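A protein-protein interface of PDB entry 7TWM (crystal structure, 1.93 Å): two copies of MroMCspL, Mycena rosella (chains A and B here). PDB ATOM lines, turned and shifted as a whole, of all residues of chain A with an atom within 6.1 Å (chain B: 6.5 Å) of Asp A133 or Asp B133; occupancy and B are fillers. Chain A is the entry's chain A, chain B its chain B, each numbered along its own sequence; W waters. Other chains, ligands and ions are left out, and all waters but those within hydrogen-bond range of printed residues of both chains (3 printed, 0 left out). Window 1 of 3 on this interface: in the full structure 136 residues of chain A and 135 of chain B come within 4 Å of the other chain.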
ATOM      1  N   HIS A 101     -32.817 -10.962 -25.486  1.00  0.00           N
ATOM      2  CA  HIS A 101     -33.518 -12.042 -26.158  1.00  0.00           C
ATOM      3  C   HIS A 101     -34.975 -11.608 -26.324  1.00  0.00           C
ATOM      4  O   HIS A 101     -35.621 -11.204 -25.357  1.00  0.00           O
ATOM      5  CB  HIS A 101     -33.395 -13.304 -25.288  1.00  0.00           C
ATOM      6  CG  HIS A 101     -33.940 -14.548 -25.903  1.00  0.00           C
ATOM      7  ND1 HIS A 101     -35.236 -14.632 -26.379  1.00  0.00           N
ATOM      8  CD2 HIS A 101     -33.400 -15.781 -26.028  1.00  0.00           C
ATOM      9  CE1 HIS A 101     -35.462 -15.861 -26.814  1.00  0.00           C
ATOM     10  NE2 HIS A 101     -34.350 -16.595 -26.580  1.00  0.00           N
ATOM     11  N   VAL A 104     -37.685 -13.241 -23.896  1.00  0.00           N
ATOM     12  CA  VAL A 104     -37.404 -13.297 -22.468  1.00  0.00           C
ATOM     13  C   VAL A 104     -37.896 -11.999 -21.833  1.00  0.00           C
ATOM     14  O   VAL A 104     -37.342 -10.930 -22.079  1.00  0.00           O
ATOM     15  CB  VAL A 104     -35.905 -13.572 -22.217  1.00  0.00           C
ATOM     16  CG1 VAL A 104     -35.472 -13.412 -20.757  1.00  0.00           C
ATOM     17  CG2 VAL A 104     -35.501 -14.932 -22.755  1.00  0.00           C
ATOM     18  N   LEU A 126     -36.043 -15.767 -33.294  1.00  0.00           N
ATOM     19  CA  LEU A 126     -34.637 -16.102 -33.155  1.00  0.00           C
ATOM     20  C   LEU A 126     -34.190 -15.754 -31.737  1.00  0.00           C
ATOM     21  O   LEU A 126     -34.644 -14.759 -31.159  1.00  0.00           O
ATOM     22  CB  LEU A 126     -33.816 -15.276 -34.148  1.00  0.00           C
ATOM     23  CG  LEU A 126     -34.225 -15.368 -35.617  1.00  0.00           C
ATOM     24  CD1 LEU A 126     -33.196 -14.658 -36.475  1.00  0.00           C
ATOM     25  CD2 LEU A 126     -34.383 -16.811 -36.058  1.00  0.00           C
ATOM     26  N   PRO A 127     -33.227 -16.503 -31.164  1.00  0.00           N
ATOM     27  CA  PRO A 127     -32.716 -16.172 -29.836  1.00  0.00           C
ATOM     28  C   PRO A 127     -31.778 -14.971 -29.925  1.00  0.00           C
ATOM     29  O   PRO A 127     -31.212 -14.685 -30.985  1.00  0.00           O
ATOM     30  CB  PRO A 127     -31.950 -17.441 -29.445  1.00  0.00           C
ATOM     31  CG  PRO A 127     -31.425 -17.966 -30.785  1.00  0.00           C
ATOM     32  CD  PRO A 127     -32.555 -17.671 -31.764  1.00  0.00           C
ATOM     33  N   GLY A 128     -31.690 -14.242 -28.804  1.00  0.00           N
ATOM     34  CA  GLY A 128     -30.743 -13.163 -28.614  1.00  0.00           C
ATOM     35  C   GLY A 128     -30.055 -13.314 -27.256  1.00  0.00           C
ATOM     36  O   GLY A 128     -30.432 -14.183 -26.462  1.00  0.00           O
ATOM     37  N   ILE A 129     -29.029 -12.490 -27.018  1.00  0.00           N
ATOM     38  CA  ILE A 129     -28.319 -12.516 -25.744  1.00  0.00           C
ATOM     39  C   ILE A 129     -29.200 -11.864 -24.678  1.00  0.00           C
ATOM     40  O   ILE A 129     -29.510 -10.687 -24.800  1.00  0.00           O
ATOM     41  CB  ILE A 129     -26.974 -11.763 -25.883  1.00  0.00           C
ATOM     42  CG1 ILE A 129     -26.062 -12.373 -26.959  1.00  0.00           C
ATOM     43  CG2 ILE A 129     -26.276 -11.612 -24.522  1.00  0.00           C
ATOM     44  CD1 ILE A 129     -25.478 -13.742 -26.605  1.00  0.00           C
ATOM     45  N   SER A 130     -29.554 -12.602 -23.608  1.00  0.00           N
ATOM     46  CA  SER A 130     -30.400 -12.067 -22.544  1.00  0.00           C
ATOM     47  C   SER A 130     -29.573 -11.407 -21.437  1.00  0.00           C
ATOM     48  O   SER A 130     -28.355 -11.570 -21.366  1.00  0.00           O
ATOM     49  CB  SER A 130     -31.264 -13.157 -21.934  1.00  0.00           C
ATOM     50  OG  SER A 130     -30.464 -13.962 -21.069  1.00  0.00           O
ATOM     51  N   ALA A 131     -30.264 -10.701 -20.524  1.00  0.00           N
ATOM     52  CA  ALA A 131     -29.607 -10.154 -19.341  1.00  0.00           C
ATOM     53  C   ALA A 131     -29.008 -11.261 -18.474  1.00  0.00           C
ATOM     54  O   ALA A 131     -28.000 -11.040 -17.811  1.00  0.00           O
ATOM     55  CB  ALA A 131     -30.557  -9.284 -18.537  1.00  0.00           C
ATOM     56  N   GLU A 132     -29.648 -12.438 -18.450  1.00  0.00           N
ATOM     57  CA  GLU A 132     -29.118 -13.581 -17.714  1.00  0.00           C
ATOM     58  C   GLU A 132     -27.809 -14.057 -18.332  1.00  0.00           C
ATOM     59  O   GLU A 132     -26.857 -14.347 -17.609  1.00  0.00           O
ATOM     60  CB  GLU A 132     -30.128 -14.728 -17.660  1.00  0.00           C
ATOM     61  CG  GLU A 132     -30.788 -14.811 -16.301  1.00  0.00           C
ATOM     62  CD  GLU A 132     -31.800 -15.929 -16.122  1.00  0.00           C
ATOM     63  OE1 GLU A 132     -31.649 -16.990 -16.786  1.00  0.00           O
ATOM     64  OE2 GLU A 132     -32.732 -15.734 -15.300  1.00  0.00           O
ATOM     65  N   ASP A 133     -27.781 -14.159 -19.669  1.00  0.00           N
ATOM     66  CA  ASP A 133     -26.554 -14.523 -20.371  1.00  0.00           C
ATOM     67  C   ASP A 133     -25.429 -13.561 -19.994  1.00  0.00           C
ATOM     68  O   ASP A 133     -24.304 -13.986 -19.749  1.00  0.00           O
ATOM     69  CB  ASP A 133     -26.724 -14.461 -21.894  1.00  0.00           C
ATOM     70  CG  ASP A 133     -27.583 -15.578 -22.449  1.00  0.00           C
ATOM     71  OD1 ASP A 133     -27.502 -16.711 -21.904  1.00  0.00           O
ATOM     72  OD2 ASP A 133     -28.348 -15.300 -23.418  1.00  0.00           O
ATOM     73  N   TYR A 134     -25.729 -12.257 -20.015  1.00  0.00           N
ATOM     74  CA  TYR A 134     -24.769 -11.220 -19.665  1.00  0.00           C
ATOM     75  C   TYR A 134     -24.315 -11.410 -18.212  1.00  0.00           C
ATOM     76  O   TYR A 134     -23.124 -11.325 -17.909  1.00  0.00           O
ATOM     77  CB  TYR A 134     -25.404  -9.845 -19.918  1.00  0.00           C
ATOM     78  CG  TYR A 134     -24.475  -8.708 -20.280  1.00  0.00           C
ATOM     79  CD1 TYR A 134     -23.107  -8.888 -20.443  1.00  0.00           C
ATOM     80  CD2 TYR A 134     -24.986  -7.439 -20.494  1.00  0.00           C
ATOM     81  CE1 TYR A 134     -22.283  -7.831 -20.810  1.00  0.00           C
ATOM     82  CE2 TYR A 134     -24.181  -6.378 -20.879  1.00  0.00           C
ATOM     83  CZ  TYR A 134     -22.818  -6.569 -21.009  1.00  0.00           C
ATOM     84  OH  TYR A 134     -22.033  -5.514 -21.373  1.00  0.00           O
ATOM     85  N   MET A 135     -25.265 -11.713 -17.319  1.00  0.00           N
ATOM     86  CA  MET A 135     -24.959 -11.902 -15.907  1.00  0.00           C
ATOM     87  C   MET A 135     -24.006 -13.084 -15.690  1.00  0.00           C
ATOM     88  O   MET A 135     -23.030 -12.953 -14.953  1.00  0.00           O
ATOM     89  CB  MET A 135     -26.242 -12.099 -15.088  1.00  0.00           C
ATOM     90  CG  MET A 135     -25.958 -12.427 -13.619  1.00  0.00           C
ATOM     91  SD  MET A 135     -27.411 -12.944 -12.668  1.00  0.00           S
ATOM     92  CE  MET A 135     -28.216 -11.362 -12.416  1.00  0.00           C
ATOM     93  N   PHE A 136     -24.270 -14.232 -16.335  1.00  0.00           N
ATOM     94  CA  PHE A 136     -23.388 -15.385 -16.186  1.00  0.00           C
ATOM     95  C   PHE A 136     -21.950 -15.015 -16.555  1.00  0.00           C
ATOM     96  O   PHE A 136     -21.004 -15.414 -15.872  1.00  0.00           O
ATOM     97  CB  PHE A 136     -23.869 -16.597 -16.998  1.00  0.00           C
ATOM     98  CG  PHE A 136     -25.292 -17.057 -16.769  1.00  0.00           C
ATOM     99  CD1 PHE A 136     -25.848 -17.089 -15.495  1.00  0.00           C
ATOM    100  CD2 PHE A 136     -26.080 -17.483 -17.834  1.00  0.00           C
ATOM    101  CE1 PHE A 136     -27.152 -17.524 -15.286  1.00  0.00           C
ATOM    102  CE2 PHE A 136     -27.377 -17.925 -17.625  1.00  0.00           C
ATOM    103  CZ  PHE A 136     -27.917 -17.937 -16.353  1.00  0.00           C
ATOM    104  N   ALA A 137     -21.793 -14.280 -17.662  1.00  0.00           N
ATOM    105  CA  ALA A 137     -20.486 -13.871 -18.146  1.00  0.00           C
ATOM    106  C   ALA A 137     -19.832 -12.875 -17.184  1.00  0.00           C
ATOM    107  O   ALA A 137     -18.640 -13.000 -16.897  1.00  0.00           O
ATOM    108  CB  ALA A 137     -20.612 -13.314 -19.544  1.00  0.00           C
ATOM    109  N   ASP A 138     -20.616 -11.915 -16.672  1.00  0.00           N
ATOM    110  CA  ASP A 138     -20.093 -10.836 -15.836  1.00  0.00           C
ATOM    111  C   ASP A 138     -19.830 -11.303 -14.403  1.00  0.00           C
ATOM    112  O   ASP A 138     -18.792 -10.971 -13.833  1.00  0.00           O
ATOM    113  CB  ASP A 138     -21.001  -9.598 -15.838  1.00  0.00           C
ATOM    114  CG  ASP A 138     -20.851  -8.735 -17.084  1.00  0.00           C
ATOM    115  OD1 ASP A 138     -19.809  -8.878 -17.756  1.00  0.00           O
ATOM    116  OD2 ASP A 138     -21.784  -7.941 -17.391  1.00  0.00           O
ATOM    117  N   TYR A 209     -27.062  -6.399 -10.131  1.00  0.00           N
ATOM    118  CA  TYR A 209     -26.412  -6.515 -11.433  1.00  0.00           C
ATOM    119  C   TYR A 209     -27.038  -5.574 -12.457  1.00  0.00           C
ATOM    120  O   TYR A 209     -28.256  -5.573 -12.662  1.00  0.00           O
ATOM    121  CB  TYR A 209     -26.415  -7.961 -11.948  1.00  0.00           C
ATOM    122  CG  TYR A 209     -25.865  -8.102 -13.350  1.00  0.00           C
ATOM    123  CD1 TYR A 209     -24.536  -7.811 -13.635  1.00  0.00           C
ATOM    124  CD2 TYR A 209     -26.685  -8.506 -14.397  1.00  0.00           C
ATOM    125  CE1 TYR A 209     -24.022  -7.931 -14.919  1.00  0.00           C
ATOM    126  CE2 TYR A 209     -26.191  -8.620 -15.689  1.00  0.00           C
ATOM    127  CZ  TYR A 209     -24.863  -8.335 -15.950  1.00  0.00           C
ATOM    128  OH  TYR A 209     -24.390  -8.468 -17.221  1.00  0.00           O
ATOM    129  N   HIS B 101     -23.169 -20.661 -24.828  1.00  0.00           N
ATOM    130  CA  HIS B 101     -22.653 -19.667 -23.902  1.00  0.00           C
ATOM    131  C   HIS B 101     -21.437 -20.257 -23.195  1.00  0.00           C
ATOM    132  O   HIS B 101     -21.541 -21.338 -22.616  1.00  0.00           O
ATOM    133  CB  HIS B 101     -23.742 -19.363 -22.858  1.00  0.00           C
ATOM    134  CG  HIS B 101     -23.422 -18.229 -21.945  1.00  0.00           C
ATOM    135  ND1 HIS B 101     -22.294 -18.216 -21.138  1.00  0.00           N
ATOM    136  CD2 HIS B 101     -24.080 -17.070 -21.707  1.00  0.00           C
ATOM    137  CE1 HIS B 101     -22.271 -17.110 -20.429  1.00  0.00           C
ATOM    138  NE2 HIS B 101     -23.367 -16.383 -20.754  1.00  0.00           N
ATOM    139  N   VAL B 104     -21.854 -21.615 -19.415  1.00  0.00           N
ATOM    140  CA  VAL B 104     -22.961 -22.487 -19.056  1.00  0.00           C
ATOM    141  C   VAL B 104     -22.530 -23.920 -19.362  1.00  0.00           C
ATOM    142  O   VAL B 104     -22.341 -24.278 -20.526  1.00  0.00           O
ATOM    143  CB  VAL B 104     -24.252 -22.082 -19.799  1.00  0.00           C
ATOM    144  CG1 VAL B 104     -25.396 -23.059 -19.543  1.00  0.00           C
ATOM    145  CG2 VAL B 104     -24.680 -20.653 -19.482  1.00  0.00           C
ATOM    146  N   LEU B 126     -17.379 -13.243 -22.580  1.00  0.00           N
ATOM    147  CA  LEU B 126     -18.458 -12.676 -23.381  1.00  0.00           C
ATOM    148  C   LEU B 126     -19.616 -13.674 -23.396  1.00  0.00           C
ATOM    149  O   LEU B 126     -19.392 -14.882 -23.539  1.00  0.00           O
ATOM    150  CB  LEU B 126     -17.994 -12.438 -24.826  1.00  0.00           C
ATOM    151  CG  LEU B 126     -16.701 -11.636 -25.028  1.00  0.00           C
ATOM    152  CD1 LEU B 126     -16.466 -11.354 -26.503  1.00  0.00           C
ATOM    153  CD2 LEU B 126     -16.723 -10.330 -24.257  1.00  0.00           C
ATOM    154  N   PRO B 127     -20.885 -13.212 -23.303  1.00  0.00           N
ATOM    155  CA  PRO B 127     -22.024 -14.128 -23.370  1.00  0.00           C
ATOM    156  C   PRO B 127     -22.182 -14.645 -24.800  1.00  0.00           C
ATOM    157  O   PRO B 127     -21.771 -13.986 -25.756  1.00  0.00           O
ATOM    158  CB  PRO B 127     -23.216 -13.230 -23.017  1.00  0.00           C
ATOM    159  CG  PRO B 127     -22.772 -11.839 -23.461  1.00  0.00           C
ATOM    160  CD  PRO B 127     -21.282 -11.800 -23.174  1.00  0.00           C
ATOM    161  N   GLY B 128     -22.761 -15.841 -24.919  1.00  0.00           N
ATOM    162  CA  GLY B 128     -23.181 -16.408 -26.188  1.00  0.00           C
ATOM    163  C   GLY B 128     -24.591 -16.973 -26.058  1.00  0.00           C
ATOM    164  O   GLY B 128     -25.135 -17.030 -24.952  1.00  0.00           O
ATOM    165  N   ILE B 129     -25.177 -17.373 -27.194  1.00  0.00           N
ATOM    166  CA  ILE B 129     -26.524 -17.923 -27.215  1.00  0.00           C
ATOM    167  C   ILE B 129     -26.474 -19.324 -26.601  1.00  0.00           C
ATOM    168  O   ILE B 129     -25.744 -20.185 -27.105  1.00  0.00           O
ATOM    169  CB  ILE B 129     -27.067 -17.992 -28.664  1.00  0.00           C
ATOM    170  CG1 ILE B 129     -27.086 -16.623 -29.363  1.00  0.00           C
ATOM    171  CG2 ILE B 129     -28.434 -18.668 -28.695  1.00  0.00           C
ATOM    172  CD1 ILE B 129     -28.017 -15.598 -28.706  1.00  0.00           C
ATOM    173  N   SER B 130     -27.311 -19.562 -25.581  1.00  0.00           N
ATOM    174  CA  SER B 130     -27.345 -20.837 -24.870  1.00  0.00           C
ATOM    175  C   SER B 130     -28.408 -21.757 -25.471  1.00  0.00           C
ATOM    176  O   SER B 130     -29.273 -21.307 -26.227  1.00  0.00           O
ATOM    177  CB  SER B 130     -27.624 -20.604 -23.404  1.00  0.00           C
ATOM    178  OG  SER B 130     -28.950 -20.119 -23.227  1.00  0.00           O
ATOM    179  N   ALA B 131     -28.359 -23.050 -25.104  1.00  0.00           N
ATOM    180  CA  ALA B 131     -29.401 -23.990 -25.502  1.00  0.00           C
ATOM    181  C   ALA B 131     -30.764 -23.513 -24.999  1.00  0.00           C
ATOM    182  O   ALA B 131     -31.778 -23.615 -25.702  1.00  0.00           O
ATOM    183  CB  ALA B 131     -29.073 -25.379 -25.014  1.00  0.00           C
ATOM    184  N   GLU B 132     -30.769 -22.973 -23.774  1.00  0.00           N
ATOM    185  CA  GLU B 132     -31.953 -22.403 -23.151  1.00  0.00           C
ATOM    186  C   GLU B 132     -32.522 -21.250 -23.990  1.00  0.00           C
ATOM    187  O   GLU B 132     -33.732 -21.166 -24.194  1.00  0.00           O
ATOM    188  CB  GLU B 132     -31.583 -21.994 -21.719  1.00  0.00           C
ATOM    189  CG  GLU B 132     -32.719 -21.404 -20.923  1.00  0.00           C
ATOM    190  CD  GLU B 132     -32.419 -21.206 -19.442  1.00  0.00           C
ATOM    191  OE1 GLU B 132     -31.232 -21.132 -19.075  1.00  0.00           O
ATOM    192  OE2 GLU B 132     -33.374 -21.141 -18.656  1.00  0.00           O
ATOM    193  N   ASP B 133     -31.651 -20.328 -24.424  1.00  0.00           N
ATOM    194  CA  ASP B 133     -32.039 -19.236 -25.308  1.00  0.00           C
ATOM    195  C   ASP B 133     -32.727 -19.765 -26.573  1.00  0.00           C
ATOM    196  O   ASP B 133     -33.746 -19.224 -26.999  1.00  0.00           O
ATOM    197  CB  ASP B 133     -30.823 -18.415 -25.738  1.00  0.00           C
ATOM    198  CG  ASP B 133     -30.283 -17.521 -24.634  1.00  0.00           C
ATOM    199  OD1 ASP B 133     -31.077 -17.150 -23.722  1.00  0.00           O
ATOM    200  OD2 ASP B 133     -29.063 -17.207 -24.683  1.00  0.00           O
ATOM    201  N   TYR B 134     -32.142 -20.805 -27.181  1.00  0.00           N
ATOM    202  CA  TYR B 134     -32.668 -21.405 -28.401  1.00  0.00           C
ATOM    203  C   TYR B 134     -34.052 -21.989 -28.118  1.00  0.00           C
ATOM    204  O   TYR B 134     -34.980 -21.812 -28.905  1.00  0.00           O
ATOM    205  CB  TYR B 134     -31.677 -22.454 -28.917  1.00  0.00           C
ATOM    206  CG  TYR B 134     -31.601 -22.706 -30.407  1.00  0.00           C
ATOM    207  CD1 TYR B 134     -32.369 -22.014 -31.338  1.00  0.00           C
ATOM    208  CD2 TYR B 134     -30.707 -23.651 -30.888  1.00  0.00           C
ATOM    209  CE1 TYR B 134     -32.256 -22.279 -32.705  1.00  0.00           C
ATOM    210  CE2 TYR B 134     -30.572 -23.908 -32.247  1.00  0.00           C
ATOM    211  CZ  TYR B 134     -31.362 -23.238 -33.160  1.00  0.00           C
ATOM    212  OH  TYR B 134     -31.189 -23.529 -34.491  1.00  0.00           O
ATOM    213  N   MET B 135     -34.182 -22.632 -26.953  1.00  0.00           N
ATOM    214  CA  MET B 135     -35.440 -23.239 -26.552  1.00  0.00           C
ATOM    215  C   MET B 135     -36.570 -22.211 -26.436  1.00  0.00           C
ATOM    216  O   MET B 135     -37.672 -22.474 -26.915  1.00  0.00           O
ATOM    217  CB  MET B 135     -35.292 -23.975 -25.215  1.00  0.00           C
ATOM    218  CG  MET B 135     -36.643 -24.516 -24.718  1.00  0.00           C
ATOM    219  SD  MET B 135     -36.568 -25.369 -23.137  1.00  0.00           S
ATOM    220  CE  MET B 135     -36.131 -27.013 -23.701  1.00  0.00           C
ATOM    221  N   PHE B 136     -36.324 -21.068 -25.766  1.00  0.00           N
ATOM    222  CA  PHE B 136     -37.373 -20.065 -25.614  1.00  0.00           C
ATOM    223  C   PHE B 136     -37.884 -19.630 -26.989  1.00  0.00           C
ATOM    224  O   PHE B 136     -39.095 -19.494 -27.191  1.00  0.00           O
ATOM    225  CB  PHE B 136     -36.875 -18.825 -24.865  1.00  0.00           C
ATOM    226  CG  PHE B 136     -36.414 -19.050 -23.447  1.00  0.00           C
ATOM    227  CD1 PHE B 136     -37.154 -19.837 -22.574  1.00  0.00           C
ATOM    228  CD2 PHE B 136     -35.257 -18.442 -22.976  1.00  0.00           C
ATOM    229  CE1 PHE B 136     -36.726 -20.045 -21.270  1.00  0.00           C
ATOM    230  CE2 PHE B 136     -34.847 -18.626 -21.661  1.00  0.00           C
ATOM    231  CZ  PHE B 136     -35.580 -19.426 -20.811  1.00  0.00           C
ATOM    232  N   ALA B 137     -36.947 -19.425 -27.924  1.00  0.00           N
ATOM    233  CA  ALA B 137     -37.285 -18.981 -29.271  1.00  0.00           C
ATOM    234  C   ALA B 137     -38.038 -20.067 -30.048  1.00  0.00           C
ATOM    235  O   ALA B 137     -39.047 -19.773 -30.693  1.00  0.00           O
ATOM    236  CB  ALA B 137     -36.047 -18.504 -30.009  1.00  0.00           C
ATOM    237  N   ASP B 138     -37.564 -21.318 -29.975  1.00  0.00           N
ATOM    238  CA  ASP B 138     -38.154 -22.389 -30.772  1.00  0.00           C
ATOM    239  C   ASP B 138     -39.483 -22.868 -30.180  1.00  0.00           C
ATOM    240  O   ASP B 138     -40.399 -23.192 -30.928  1.00  0.00           O
ATOM    241  CB  ASP B 138     -37.196 -23.576 -30.936  1.00  0.00           C
ATOM    242  CG  ASP B 138     -36.113 -23.391 -31.985  1.00  0.00           C
ATOM    243  OD1 ASP B 138     -36.278 -22.506 -32.830  1.00  0.00           O
ATOM    244  OD2 ASP B 138     -35.075 -24.115 -31.914  1.00  0.00           O
ATOM    245  N   TYR B 209     -36.800 -31.320 -26.747  1.00  0.00           N
ATOM    246  CA  TYR B 209     -36.277 -30.242 -27.569  1.00  0.00           C
ATOM    247  C   TYR B 209     -34.839 -30.531 -27.998  1.00  0.00           C
ATOM    248  O   TYR B 209     -33.993 -30.840 -27.158  1.00  0.00           O
ATOM    249  CB  TYR B 209     -36.361 -28.903 -26.824  1.00  0.00           C
ATOM    250  CG  TYR B 209     -35.690 -27.777 -27.571  1.00  0.00           C
ATOM    251  CD1 TYR B 209     -36.173 -27.363 -28.800  1.00  0.00           C
ATOM    252  CD2 TYR B 209     -34.548 -27.161 -27.080  1.00  0.00           C
ATOM    253  CE1 TYR B 209     -35.553 -26.352 -29.520  1.00  0.00           C
ATOM    254  CE2 TYR B 209     -33.915 -26.145 -27.786  1.00  0.00           C
ATOM    255  CZ  TYR B 209     -34.420 -25.743 -29.009  1.00  0.00           C
ATOM    256  OH  TYR B 209     -33.832 -24.730 -29.707  1.00  0.00           O
HETATM  257  O   HOH W   1     -28.900 -18.824 -20.959  1.00  0.00           O
HETATM  258  O   HOH W   2     -31.490 -16.357 -21.203  1.00  0.00           O
HETATM  259  O   HOH W   3     -31.020 -18.136 -19.019  1.00  0.00           O
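NE2 of His A101 sits at hydrogen-bond distance from O of Asp B133.
The backbone carbonyl oxygen of Asp A133 sits at hydrogen-bond distance from a ring nitrogen (NE2) of His B101, at 2.8 Å.
OD2 of Asp A133 lies close to OD2 of Asp B133, at 2.4 Å.
The backbone NH of His A101 sits at hydrogen-bond distance from the backbone carbonyl oxygen of Ile A129, at 3.4 Å.
OD2 of Asp A133 sits at hydrogen-bond distance from N of Ser A130, 3.0 Å away.
The backbone carbonyl oxygen of Ile B129 is in hydrogen-bond range of the backbone NH of His B101 (3.5 Å).
The backbone NH of Glu B132 lies close to the side-chain hydroxyl of Ser B130 (3.4 Å).
OG of Ser B130 sits at hydrogen-bond distance from N of Asp B133.
Ile B129 touches Pro A127 (CG2 to CG, 3.7 Å).
Gly A128 touches Ile B129 (C to CD1, 3.4 Å).
O of Gly A128 touches OD2 of Asp B133 (3.8 Å).
Ile A129 touches Gly B128.
Pro B127 touches Asp A133 (CB to O, 3.5 Å).
OG of Ser B130 touches OD1 of Asp A133 (3.9 Å).
Phe A136 touches His B101 (CB to NE2, 3.8 Å).
Phe A136 touches Val B104.
Ala A137 touches His B101.
Pro B127 touches Ala A137 (N to CB, 3.8 Å).
Of the printed residues of chain B, Ile A129 touches Pro B127, Gly B128 and Ile B129.
Ala A131 touches none of the printed residues of chain B.
Of chain B, only His B101 (2.8 Å), Pro B127 (3.5 Å), Gly B128 (3.8 Å), Ser B130 (3.9 Å) and Asp B133 (2.4 Å) come within 4 Å of Asp A133.
Of the printed residues of chain A, Pro B127 touches Ile A129 (3.7 Å), Asp A133 (3.5 Å) and Ala A137 (3.8 Å).
Of the printed residues of chain A, Ser B130 touches Asp A133 (3.9 Å).
Met B135 touches none of the printed residues of chain A.
Hydrophobic or aromatic side chains of chain A that line the printed part of chain B: His A101, Val A104, Pro A127, Ile A129, Phe A136 and Ala A137.
Of the 16 printed residues of chain B, 10 touch a printed residue of chain A.
Hydrophobic or aromatic side chains of chain B within 4 Å of the printed part of chain A: His B101, Val B104, Pro B127, Ile B129, Phe B136 and Ala B137.
Among the printed residues, 22 pairs touch across the chains.
Leu A126 touches Ala B137, and with the chains exchanged Ala A137 touches Leu B126.
Pro A127 touches Asp B133, and with the chains exchanged Asp A133 touches Pro B127.
Gly A128 touches Asp B133, and with the chains exchanged Asp A133 touches Gly B128.
Ala A137 touches His B101, but with the chains exchanged His A101 does not touch Ala B137 (4.02 Å).
16 positions are printed for both chains.
Water W3 bridges OE1 of Glu A132 (2.6 Å) and OE1 of Glu B132 (3.0 Å).
Water W2 bridges OG of Ser A130 (2.6 Å) and OD1 of Asp B133 (2.7 Å).
Water W1 lies within hydrogen-bond range of OG of Ser B130 (2.6 Å) and OD1 of Asp A133 (2.7 Å).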
